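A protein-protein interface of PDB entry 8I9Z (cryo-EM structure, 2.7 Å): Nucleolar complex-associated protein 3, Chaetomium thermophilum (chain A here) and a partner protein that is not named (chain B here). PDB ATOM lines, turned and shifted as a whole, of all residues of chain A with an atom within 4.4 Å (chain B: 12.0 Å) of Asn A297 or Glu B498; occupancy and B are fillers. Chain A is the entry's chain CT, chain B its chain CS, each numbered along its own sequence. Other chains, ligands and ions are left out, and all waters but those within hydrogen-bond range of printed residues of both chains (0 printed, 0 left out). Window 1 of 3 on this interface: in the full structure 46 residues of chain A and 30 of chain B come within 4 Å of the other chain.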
ATOM      1  N   ARG A 183       7.706  36.974  10.871  1.00  0.00           N
ATOM      2  CA  ARG A 183       6.367  37.274  11.349  1.00  0.00           C
ATOM      3  C   ARG A 183       6.436  37.850  12.753  1.00  0.00           C
ATOM      4  O   ARG A 183       7.411  37.650  13.483  1.00  0.00           O
ATOM      5  CB  ARG A 183       5.505  36.016  11.350  1.00  0.00           C
ATOM      6  CG  ARG A 183       5.078  35.575   9.980  1.00  0.00           C
ATOM      7  CD  ARG A 183       4.219  34.332  10.035  1.00  0.00           C
ATOM      8  NE  ARG A 183       3.436  34.159   8.818  1.00  0.00           N
ATOM      9  CZ  ARG A 183       2.296  33.487   8.751  1.00  0.00           C
ATOM     10  NH1 ARG A 183       1.772  32.909   9.817  1.00  0.00           N
ATOM     11  NH2 ARG A 183       1.666  33.397   7.584  1.00  0.00           N
ATOM     12  N   ARG A 185       4.235  38.367  16.430  1.00  0.00           N
ATOM     13  CA  ARG A 185       3.142  37.824  17.217  1.00  0.00           C
ATOM     14  C   ARG A 185       2.217  38.946  17.682  1.00  0.00           C
ATOM     15  O   ARG A 185       2.647  40.097  17.791  1.00  0.00           O
ATOM     16  CB  ARG A 185       3.693  37.076  18.430  1.00  0.00           C
ATOM     17  CG  ARG A 185       5.154  36.666  18.310  1.00  0.00           C
ATOM     18  CD  ARG A 185       5.306  35.176  18.077  1.00  0.00           C
ATOM     19  NE  ARG A 185       4.430  34.412  18.956  1.00  0.00           N
ATOM     20  CZ  ARG A 185       3.936  33.214  18.673  1.00  0.00           C
ATOM     21  NH1 ARG A 185       4.231  32.594  17.544  1.00  0.00           N
ATOM     22  NH2 ARG A 185       3.131  32.622  19.551  1.00  0.00           N
ATOM     23  N   ARG A 259      -0.778  35.468   4.498  1.00  0.00           N
ATOM     24  CA  ARG A 259      -0.518  34.989   3.145  1.00  0.00           C
ATOM     25  C   ARG A 259      -1.688  34.182   2.611  1.00  0.00           C
ATOM     26  O   ARG A 259      -1.860  34.079   1.392  1.00  0.00           O
ATOM     27  CB  ARG A 259       0.762  34.160   3.091  1.00  0.00           C
ATOM     28  CG  ARG A 259       0.894  33.114   4.165  1.00  0.00           C
ATOM     29  CD  ARG A 259       1.947  32.087   3.781  1.00  0.00           C
ATOM     30  NE  ARG A 259       1.791  30.848   4.530  1.00  0.00           N
ATOM     31  CZ  ARG A 259       2.792  30.186   5.091  1.00  0.00           C
ATOM     32  NH1 ARG A 259       4.041  30.610   4.995  1.00  0.00           N
ATOM     33  NH2 ARG A 259       2.533  29.072   5.769  1.00  0.00           N
ATOM     34  N   ASP A 293      10.059  28.245  -3.441  1.00  0.00           N
ATOM     35  CA  ASP A 293       9.881  28.044  -2.010  1.00  0.00           C
ATOM     36  C   ASP A 293      10.609  26.774  -1.587  1.00  0.00           C
ATOM     37  O   ASP A 293      10.346  25.690  -2.113  1.00  0.00           O
ATOM     38  CB  ASP A 293       8.386  27.969  -1.682  1.00  0.00           C
ATOM     39  CG  ASP A 293       8.078  27.356  -0.317  1.00  0.00           C
ATOM     40  OD1 ASP A 293       6.960  26.824  -0.173  1.00  0.00           O
ATOM     41  OD2 ASP A 293       8.868  27.494   0.642  1.00  0.00           O
ATOM     42  N   GLU A 295      11.313  26.166   2.068  1.00  0.00           N
ATOM     43  CA  GLU A 295      10.818  25.737   3.371  1.00  0.00           C
ATOM     44  C   GLU A 295       9.567  24.881   3.231  1.00  0.00           C
ATOM     45  O   GLU A 295       9.432  23.853   3.904  1.00  0.00           O
ATOM     46  CB  GLU A 295      10.539  26.960   4.241  1.00  0.00           C
ATOM     47  CG  GLU A 295      11.771  27.807   4.515  1.00  0.00           C
ATOM     48  CD  GLU A 295      11.651  28.623   5.787  1.00  0.00           C
ATOM     49  OE1 GLU A 295      10.520  29.029   6.128  1.00  0.00           O
ATOM     50  OE2 GLU A 295      12.688  28.868   6.440  1.00  0.00           O
ATOM     51  N   GLY A 296       8.644  25.287   2.367  1.00  0.00           N
ATOM     52  CA  GLY A 296       7.472  24.501   2.063  1.00  0.00           C
ATOM     53  C   GLY A 296       6.191  24.960   2.716  1.00  0.00           C
ATOM     54  O   GLY A 296       5.126  24.432   2.378  1.00  0.00           O
ATOM     55  N   ASN A 297       6.257  25.909   3.649  1.00  0.00           N
ATOM     56  CA  ASN A 297       5.039  26.374   4.301  1.00  0.00           C
ATOM     57  C   ASN A 297       4.158  27.153   3.338  1.00  0.00           C
ATOM     58  O   ASN A 297       2.929  27.040   3.385  1.00  0.00           O
ATOM     59  CB  ASN A 297       5.384  27.224   5.519  1.00  0.00           C
ATOM     60  CG  ASN A 297       6.323  26.522   6.464  1.00  0.00           C
ATOM     61  OD1 ASN A 297       5.896  25.740   7.309  1.00  0.00           O
ATOM     62  ND2 ASN A 297       7.613  26.798   6.330  1.00  0.00           N
ATOM     63  N   ALA A 298       4.766  27.943   2.454  1.00  0.00           N
ATOM     64  CA  ALA A 298       3.986  28.699   1.484  1.00  0.00           C
ATOM     65  C   ALA A 298       3.351  27.777   0.455  1.00  0.00           C
ATOM     66  O   ALA A 298       2.222  28.015   0.013  1.00  0.00           O
ATOM     67  CB  ALA A 298       4.871  29.740   0.802  1.00  0.00           C
ATOM     68  N   SER A 299       4.053  26.707   0.079  1.00  0.00           N
ATOM     69  CA  SER A 299       3.533  25.790  -0.928  1.00  0.00           C
ATOM     70  C   SER A 299       2.363  24.983  -0.394  1.00  0.00           C
ATOM     71  O   SER A 299       1.412  24.704  -1.129  1.00  0.00           O
ATOM     72  CB  SER A 299       4.641  24.862  -1.410  1.00  0.00           C
ATOM     73  OG  SER A 299       5.303  25.410  -2.537  1.00  0.00           O
ATOM     74  N   GLN A 300       2.413  24.604   0.884  1.00  0.00           N
ATOM     75  CA  GLN A 300       1.341  23.809   1.474  1.00  0.00           C
ATOM     76  C   GLN A 300       0.032  24.583   1.528  1.00  0.00           C
ATOM     77  O   GLN A 300      -1.033  24.030   1.237  1.00  0.00           O
ATOM     78  CB  GLN A 300       1.749  23.350   2.871  1.00  0.00           C
ATOM     79  CG  GLN A 300       0.661  22.648   3.651  1.00  0.00           C
ATOM     80  CD  GLN A 300       1.048  22.437   5.093  1.00  0.00           C
ATOM     81  OE1 GLN A 300       2.002  23.038   5.580  1.00  0.00           O
ATOM     82  NE2 GLN A 300       0.308  21.584   5.788  1.00  0.00           N
ATOM     83  N   GLU A 301       0.090  25.866   1.891  1.00  0.00           N
ATOM     84  CA  GLU A 301      -1.135  26.655   1.973  1.00  0.00           C
ATOM     85  C   GLU A 301      -1.708  26.930   0.590  1.00  0.00           C
ATOM     86  O   GLU A 301      -2.924  27.078   0.433  1.00  0.00           O
ATOM     87  CB  GLU A 301      -0.875  27.962   2.719  1.00  0.00           C
ATOM     88  CG  GLU A 301      -2.136  28.619   3.257  1.00  0.00           C
ATOM     89  CD  GLU A 301      -1.846  29.669   4.308  1.00  0.00           C
ATOM     90  OE1 GLU A 301      -1.420  30.782   3.938  1.00  0.00           O
ATOM     91  OE2 GLU A 301      -2.043  29.383   5.507  1.00  0.00           O
ATOM     92  N   TYR B 490      14.264  21.817  20.433  1.00  0.00           N
ATOM     93  CA  TYR B 490      13.074  22.645  20.594  1.00  0.00           C
ATOM     94  C   TYR B 490      13.370  24.098  20.245  1.00  0.00           C
ATOM     95  O   TYR B 490      12.496  24.806  19.730  1.00  0.00           O
ATOM     96  CB  TYR B 490      12.512  22.460  22.019  1.00  0.00           C
ATOM     97  CG  TYR B 490      11.297  23.286  22.456  1.00  0.00           C
ATOM     98  CD1 TYR B 490      10.139  22.645  22.866  1.00  0.00           C
ATOM     99  CD2 TYR B 490      11.355  24.667  22.631  1.00  0.00           C
ATOM    100  CE1 TYR B 490       9.035  23.355  23.285  1.00  0.00           C
ATOM    101  CE2 TYR B 490      10.262  25.383  23.059  1.00  0.00           C
ATOM    102  CZ  TYR B 490       9.109  24.723  23.395  1.00  0.00           C
ATOM    103  OH  TYR B 490       8.020  25.437  23.835  1.00  0.00           O
ATOM    104  N   ARG B 491      14.595  24.563  20.502  1.00  0.00           N
ATOM    105  CA  ARG B 491      14.954  25.924  20.112  1.00  0.00           C
ATOM    106  C   ARG B 491      14.983  26.066  18.597  1.00  0.00           C
ATOM    107  O   ARG B 491      14.673  27.135  18.058  1.00  0.00           O
ATOM    108  CB  ARG B 491      16.304  26.311  20.713  1.00  0.00           C
ATOM    109  CG  ARG B 491      16.310  26.345  22.224  1.00  0.00           C
ATOM    110  CD  ARG B 491      17.551  27.016  22.784  1.00  0.00           C
ATOM    111  NE  ARG B 491      18.350  26.081  23.565  1.00  0.00           N
ATOM    112  CZ  ARG B 491      19.624  25.803  23.331  1.00  0.00           C
ATOM    113  NH1 ARG B 491      20.311  26.444  22.404  1.00  0.00           N
ATOM    114  NH2 ARG B 491      20.229  24.876  24.065  1.00  0.00           N
ATOM    115  N   ALA B 492      15.353  24.997  17.893  1.00  0.00           N
ATOM    116  CA  ALA B 492      15.322  25.024  16.438  1.00  0.00           C
ATOM    117  C   ALA B 492      13.897  24.921  15.915  1.00  0.00           C
ATOM    118  O   ALA B 492      13.553  25.555  14.911  1.00  0.00           O
ATOM    119  CB  ALA B 492      16.186  23.898  15.876  1.00  0.00           C
ATOM    120  N   LYS B 493      13.055  24.122  16.576  1.00  0.00           N
ATOM    121  CA  LYS B 493      11.671  23.985  16.135  1.00  0.00           C
ATOM    122  C   LYS B 493      10.881  25.262  16.377  1.00  0.00           C
ATOM    123  O   LYS B 493      10.045  25.647  15.554  1.00  0.00           O
ATOM    124  CB  LYS B 493      10.999  22.806  16.834  1.00  0.00           C
ATOM    125  CG  LYS B 493      11.488  21.452  16.374  1.00  0.00           C
ATOM    126  CD  LYS B 493      10.657  20.332  16.970  1.00  0.00           C
ATOM    127  CE  LYS B 493       9.235  20.362  16.435  1.00  0.00           C
ATOM    128  NZ  LYS B 493       9.197  20.536  14.957  1.00  0.00           N
ATOM    129  N   ARG B 494      11.131  25.930  17.503  1.00  0.00           N
ATOM    130  CA  ARG B 494      10.414  27.161  17.818  1.00  0.00           C
ATOM    131  C   ARG B 494      10.816  28.298  16.887  1.00  0.00           C
ATOM    132  O   ARG B 494       9.987  29.147  16.545  1.00  0.00           O
ATOM    133  CB  ARG B 494      10.666  27.545  19.272  1.00  0.00           C
ATOM    134  CG  ARG B 494       9.643  28.498  19.860  1.00  0.00           C
ATOM    135  CD  ARG B 494       9.879  28.815  21.366  1.00  0.00           C
ATOM    136  NE  ARG B 494      11.237  28.980  21.906  1.00  0.00           N
ATOM    137  CZ  ARG B 494      12.272  29.619  21.362  1.00  0.00           C
ATOM    138  NH1 ARG B 494      12.144  30.380  20.285  1.00  0.00           N
ATOM    139  NH2 ARG B 494      13.462  29.533  21.947  1.00  0.00           N
ATOM    140  N   ALA B 495      12.086  28.338  16.480  1.00  0.00           N
ATOM    141  CA  ALA B 495      12.547  29.399  15.590  1.00  0.00           C
ATOM    142  C   ALA B 495      11.961  29.245  14.193  1.00  0.00           C
ATOM    143  O   ALA B 495      11.633  30.240  13.536  1.00  0.00           O
ATOM    144  CB  ALA B 495      14.073  29.410  15.536  1.00  0.00           C
ATOM    145  N   ARG B 496      11.823  28.008  13.719  1.00  0.00           N
ATOM    146  CA  ARG B 496      11.246  27.766  12.405  1.00  0.00           C
ATOM    147  C   ARG B 496       9.727  27.710  12.429  1.00  0.00           C
ATOM    148  O   ARG B 496       9.109  27.711  11.358  1.00  0.00           O
ATOM    149  CB  ARG B 496      11.790  26.463  11.819  1.00  0.00           C
ATOM    150  CG  ARG B 496      13.120  26.617  11.117  1.00  0.00           C
ATOM    151  CD  ARG B 496      13.665  25.273  10.669  1.00  0.00           C
ATOM    152  NE  ARG B 496      13.600  25.105   9.222  1.00  0.00           N
ATOM    153  CZ  ARG B 496      14.418  25.691   8.355  1.00  0.00           C
ATOM    154  NH1 ARG B 496      15.414  26.465   8.755  1.00  0.00           N
ATOM    155  NH2 ARG B 496      14.240  25.480   7.055  1.00  0.00           N
ATOM    156  N   GLN B 497       9.116  27.653  13.607  1.00  0.00           N
ATOM    157  CA  GLN B 497       7.666  27.614  13.695  1.00  0.00           C
ATOM    158  C   GLN B 497       7.071  28.962  13.313  1.00  0.00           C
ATOM    159  O   GLN B 497       7.597  30.023  13.660  1.00  0.00           O
ATOM    160  CB  GLN B 497       7.224  27.232  15.106  1.00  0.00           C
ATOM    161  CG  GLN B 497       5.852  26.590  15.171  1.00  0.00           C
ATOM    162  CD  GLN B 497       5.325  26.497  16.586  1.00  0.00           C
ATOM    163  OE1 GLN B 497       6.093  26.517  17.548  1.00  0.00           O
ATOM    164  NE2 GLN B 497       4.009  26.397  16.724  1.00  0.00           N
ATOM    165  N   GLU B 498       5.967  28.910  12.588  1.00  0.00           N
ATOM    166  CA  GLU B 498       5.270  30.101  12.146  1.00  0.00           C
ATOM    167  C   GLU B 498       4.257  30.518  13.206  1.00  0.00           C
ATOM    168  O   GLU B 498       4.107  29.870  14.246  1.00  0.00           O
ATOM    169  CB  GLU B 498       4.606  29.843  10.794  1.00  0.00           C
ATOM    170  CG  GLU B 498       5.492  30.136   9.602  1.00  0.00           C
ATOM    171  CD  GLU B 498       4.737  30.092   8.291  1.00  0.00           C
ATOM    172  OE1 GLU B 498       3.489  30.116   8.323  1.00  0.00           O
ATOM    173  OE2 GLU B 498       5.390  30.038   7.228  1.00  0.00           O
ATOM    174  N   VAL B 499       3.550  31.611  12.945  1.00  0.00           N
ATOM    175  CA  VAL B 499       2.454  32.025  13.806  1.00  0.00           C
ATOM    176  C   VAL B 499       1.167  31.631  13.099  1.00  0.00           C
ATOM    177  O   VAL B 499       1.187  31.250  11.923  1.00  0.00           O
ATOM    178  CB  VAL B 499       2.498  33.533  14.110  1.00  0.00           C
ATOM    179  CG1 VAL B 499       3.910  33.960  14.467  1.00  0.00           C
ATOM    180  CG2 VAL B 499       1.967  34.342  12.936  1.00  0.00           C
ATOM    181  N   ASP B 500       0.046  31.708  13.801  1.00  0.00           N
ATOM    182  CA  ASP B 500      -1.245  31.343  13.244  1.00  0.00           C
ATOM    183  C   ASP B 500      -2.053  32.603  12.983  1.00  0.00           C
ATOM    184  O   ASP B 500      -2.065  33.519  13.812  1.00  0.00           O
ATOM    185  CB  ASP B 500      -2.009  30.412  14.188  1.00  0.00           C
ATOM    186  CG  ASP B 500      -2.914  29.447  13.449  1.00  0.00           C
ATOM    187  OD1 ASP B 500      -3.000  29.543  12.208  1.00  0.00           O
ATOM    188  OD2 ASP B 500      -3.544  28.596  14.113  1.00  0.00           O
ATOM    189  N   ASP B 501      -2.715  32.652  11.826  1.00  0.00           N
ATOM    190  CA  ASP B 501      -3.691  33.708  11.581  1.00  0.00           C
ATOM    191  C   ASP B 501      -4.912  33.546  12.473  1.00  0.00           C
ATOM    192  O   ASP B 501      -5.634  34.517  12.726  1.00  0.00           O
ATOM    193  CB  ASP B 501      -4.098  33.708  10.111  1.00  0.00           C
ATOM    194  CG  ASP B 501      -3.040  34.306   9.218  1.00  0.00           C
ATOM    195  OD1 ASP B 501      -1.914  34.534   9.702  1.00  0.00           O
ATOM    196  OD2 ASP B 501      -3.331  34.539   8.027  1.00  0.00           O
ATOM    197  N   GLU B 502      -5.157  32.329  12.963  1.00  0.00           N
ATOM    198  CA  GLU B 502      -6.191  32.096  13.962  1.00  0.00           C
ATOM    199  C   GLU B 502      -5.815  32.686  15.316  1.00  0.00           C
ATOM    200  O   GLU B 502      -6.659  32.739  16.216  1.00  0.00           O
ATOM    201  CB  GLU B 502      -6.447  30.592  14.089  1.00  0.00           C
ATOM    202  CG  GLU B 502      -7.836  30.206  14.573  1.00  0.00           C
ATOM    203  CD  GLU B 502      -7.992  28.706  14.739  1.00  0.00           C
ATOM    204  OE1 GLU B 502      -7.547  27.959  13.842  1.00  0.00           O
ATOM    205  OE2 GLU B 502      -8.552  28.272  15.767  1.00  0.00           O
ATOM    206  N   GLU B 503      -4.561  33.101  15.490  1.00  0.00           N
ATOM    207  CA  GLU B 503      -4.135  33.808  16.687  1.00  0.00           C
ATOM    208  C   GLU B 503      -4.222  35.318  16.509  1.00  0.00           C
ATOM    209  O   GLU B 503      -4.525  36.037  17.469  1.00  0.00           O
ATOM    210  CB  GLU B 503      -2.709  33.375  17.052  1.00  0.00           C
ATOM    211  CG  GLU B 503      -1.978  34.238  18.064  1.00  0.00           C
ATOM    212  CD  GLU B 503      -0.517  33.859  18.205  1.00  0.00           C
ATOM    213  OE1 GLU B 503      -0.040  33.020  17.413  1.00  0.00           O
ATOM    214  OE2 GLU B 503       0.156  34.402  19.107  1.00  0.00           O
ATOM    215  N   TRP B 504      -4.031  35.804  15.285  1.00  0.00           N
ATOM    216  CA  TRP B 504      -4.042  37.232  15.001  1.00  0.00           C
ATOM    217  C   TRP B 504      -5.440  37.795  14.800  1.00  0.00           C
ATOM    218  O   TRP B 504      -5.562  38.977  14.464  1.00  0.00           O
ATOM    219  CB  TRP B 504      -3.206  37.523  13.754  1.00  0.00           C
ATOM    220  CG  TRP B 504      -1.886  38.154  14.032  1.00  0.00           C
ATOM    221  CD1 TRP B 504      -0.658  37.611  13.796  1.00  0.00           C
ATOM    222  CD2 TRP B 504      -1.652  39.449  14.591  1.00  0.00           C
ATOM    223  NE1 TRP B 504       0.327  38.486  14.177  1.00  0.00           N
ATOM    224  CE2 TRP B 504      -0.257  39.624  14.667  1.00  0.00           C
ATOM    225  CE3 TRP B 504      -2.486  40.478  15.031  1.00  0.00           C
ATOM    226  CZ2 TRP B 504       0.322  40.785  15.168  1.00  0.00           C
ATOM    227  CZ3 TRP B 504      -1.910  41.628  15.527  1.00  0.00           C
ATOM    228  CH2 TRP B 504      -0.521  41.773  15.593  1.00  0.00           C
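The guanidinium group (NH2) of Arg A259 sits at hydrogen-bond distance from the backbone carbonyl oxygen (O) of Asn A297, 3.2 Å away. The side-chain carboxylate (OE1) of Glu A301 lies within salt-bridge range of the guanidinium group (NE) of Arg A259 (3.3 Å). The backbone NH (N) of Glu A295 sits at hydrogen-bond distance from the side-chain carboxylate (OD2) of Asp A293.
The side-chain carboxylate (OE2) of Glu A295 lies within salt-bridge range of the guanidinium group (NH2) of Arg B496. The side-chain carboxylate (OE1) of Glu B498 lies within salt-bridge range of the guanidinium group (NH1) of Arg A183. The side-chain carboxylate (OE2) of Glu B498 lies within salt-bridge range of the guanidinium group (NH1) of Arg A259, at 2.7 Å. The guanidinium group (NH1) of Arg A183 is in hydrogen-bond range of the backbone carbonyl oxygen (O) of Val B499, at 2.7 Å. The side-chain carboxylate (OE2) of Glu B503 lies within salt-bridge range of the guanidinium group (NH2) of Arg A185, at 3.5 Å.
Val B499 touches Arg A185 (CG1 to NH1, 3.4 Å). Arg A185 touches Trp B504 (O to CZ2, 3.6 Å). OE2 of Glu B498 touches CB of Asn A297, 3.3 Å away.
Of the printed residues of chain B, Arg A185 touches Val B499, Glu B503 and Trp B504. Of chain B, only Arg B496 comes within 4 Å of Glu A295. Ser A299 touches none of the printed residues of chain B. Glu B498 touches three residues of chain A. Of the printed residues of chain A, Trp B504 touches Arg A185 (3.6 Å). The nearest residue of chain B that does not touch Asn A297 is Arg B496 (5.3 Å). The nearest residue of chain A that does not touch Glu B498 is Arg A185 (4.3 Å). The nearest printed residue of chain A that does not touch Arg B496 is Asn A297 (5.3 Å).
Of the 11 printed residues of chain A, 5 touch a printed residue of chain B. Among the printed residues, 8 pairs touch across the chains.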
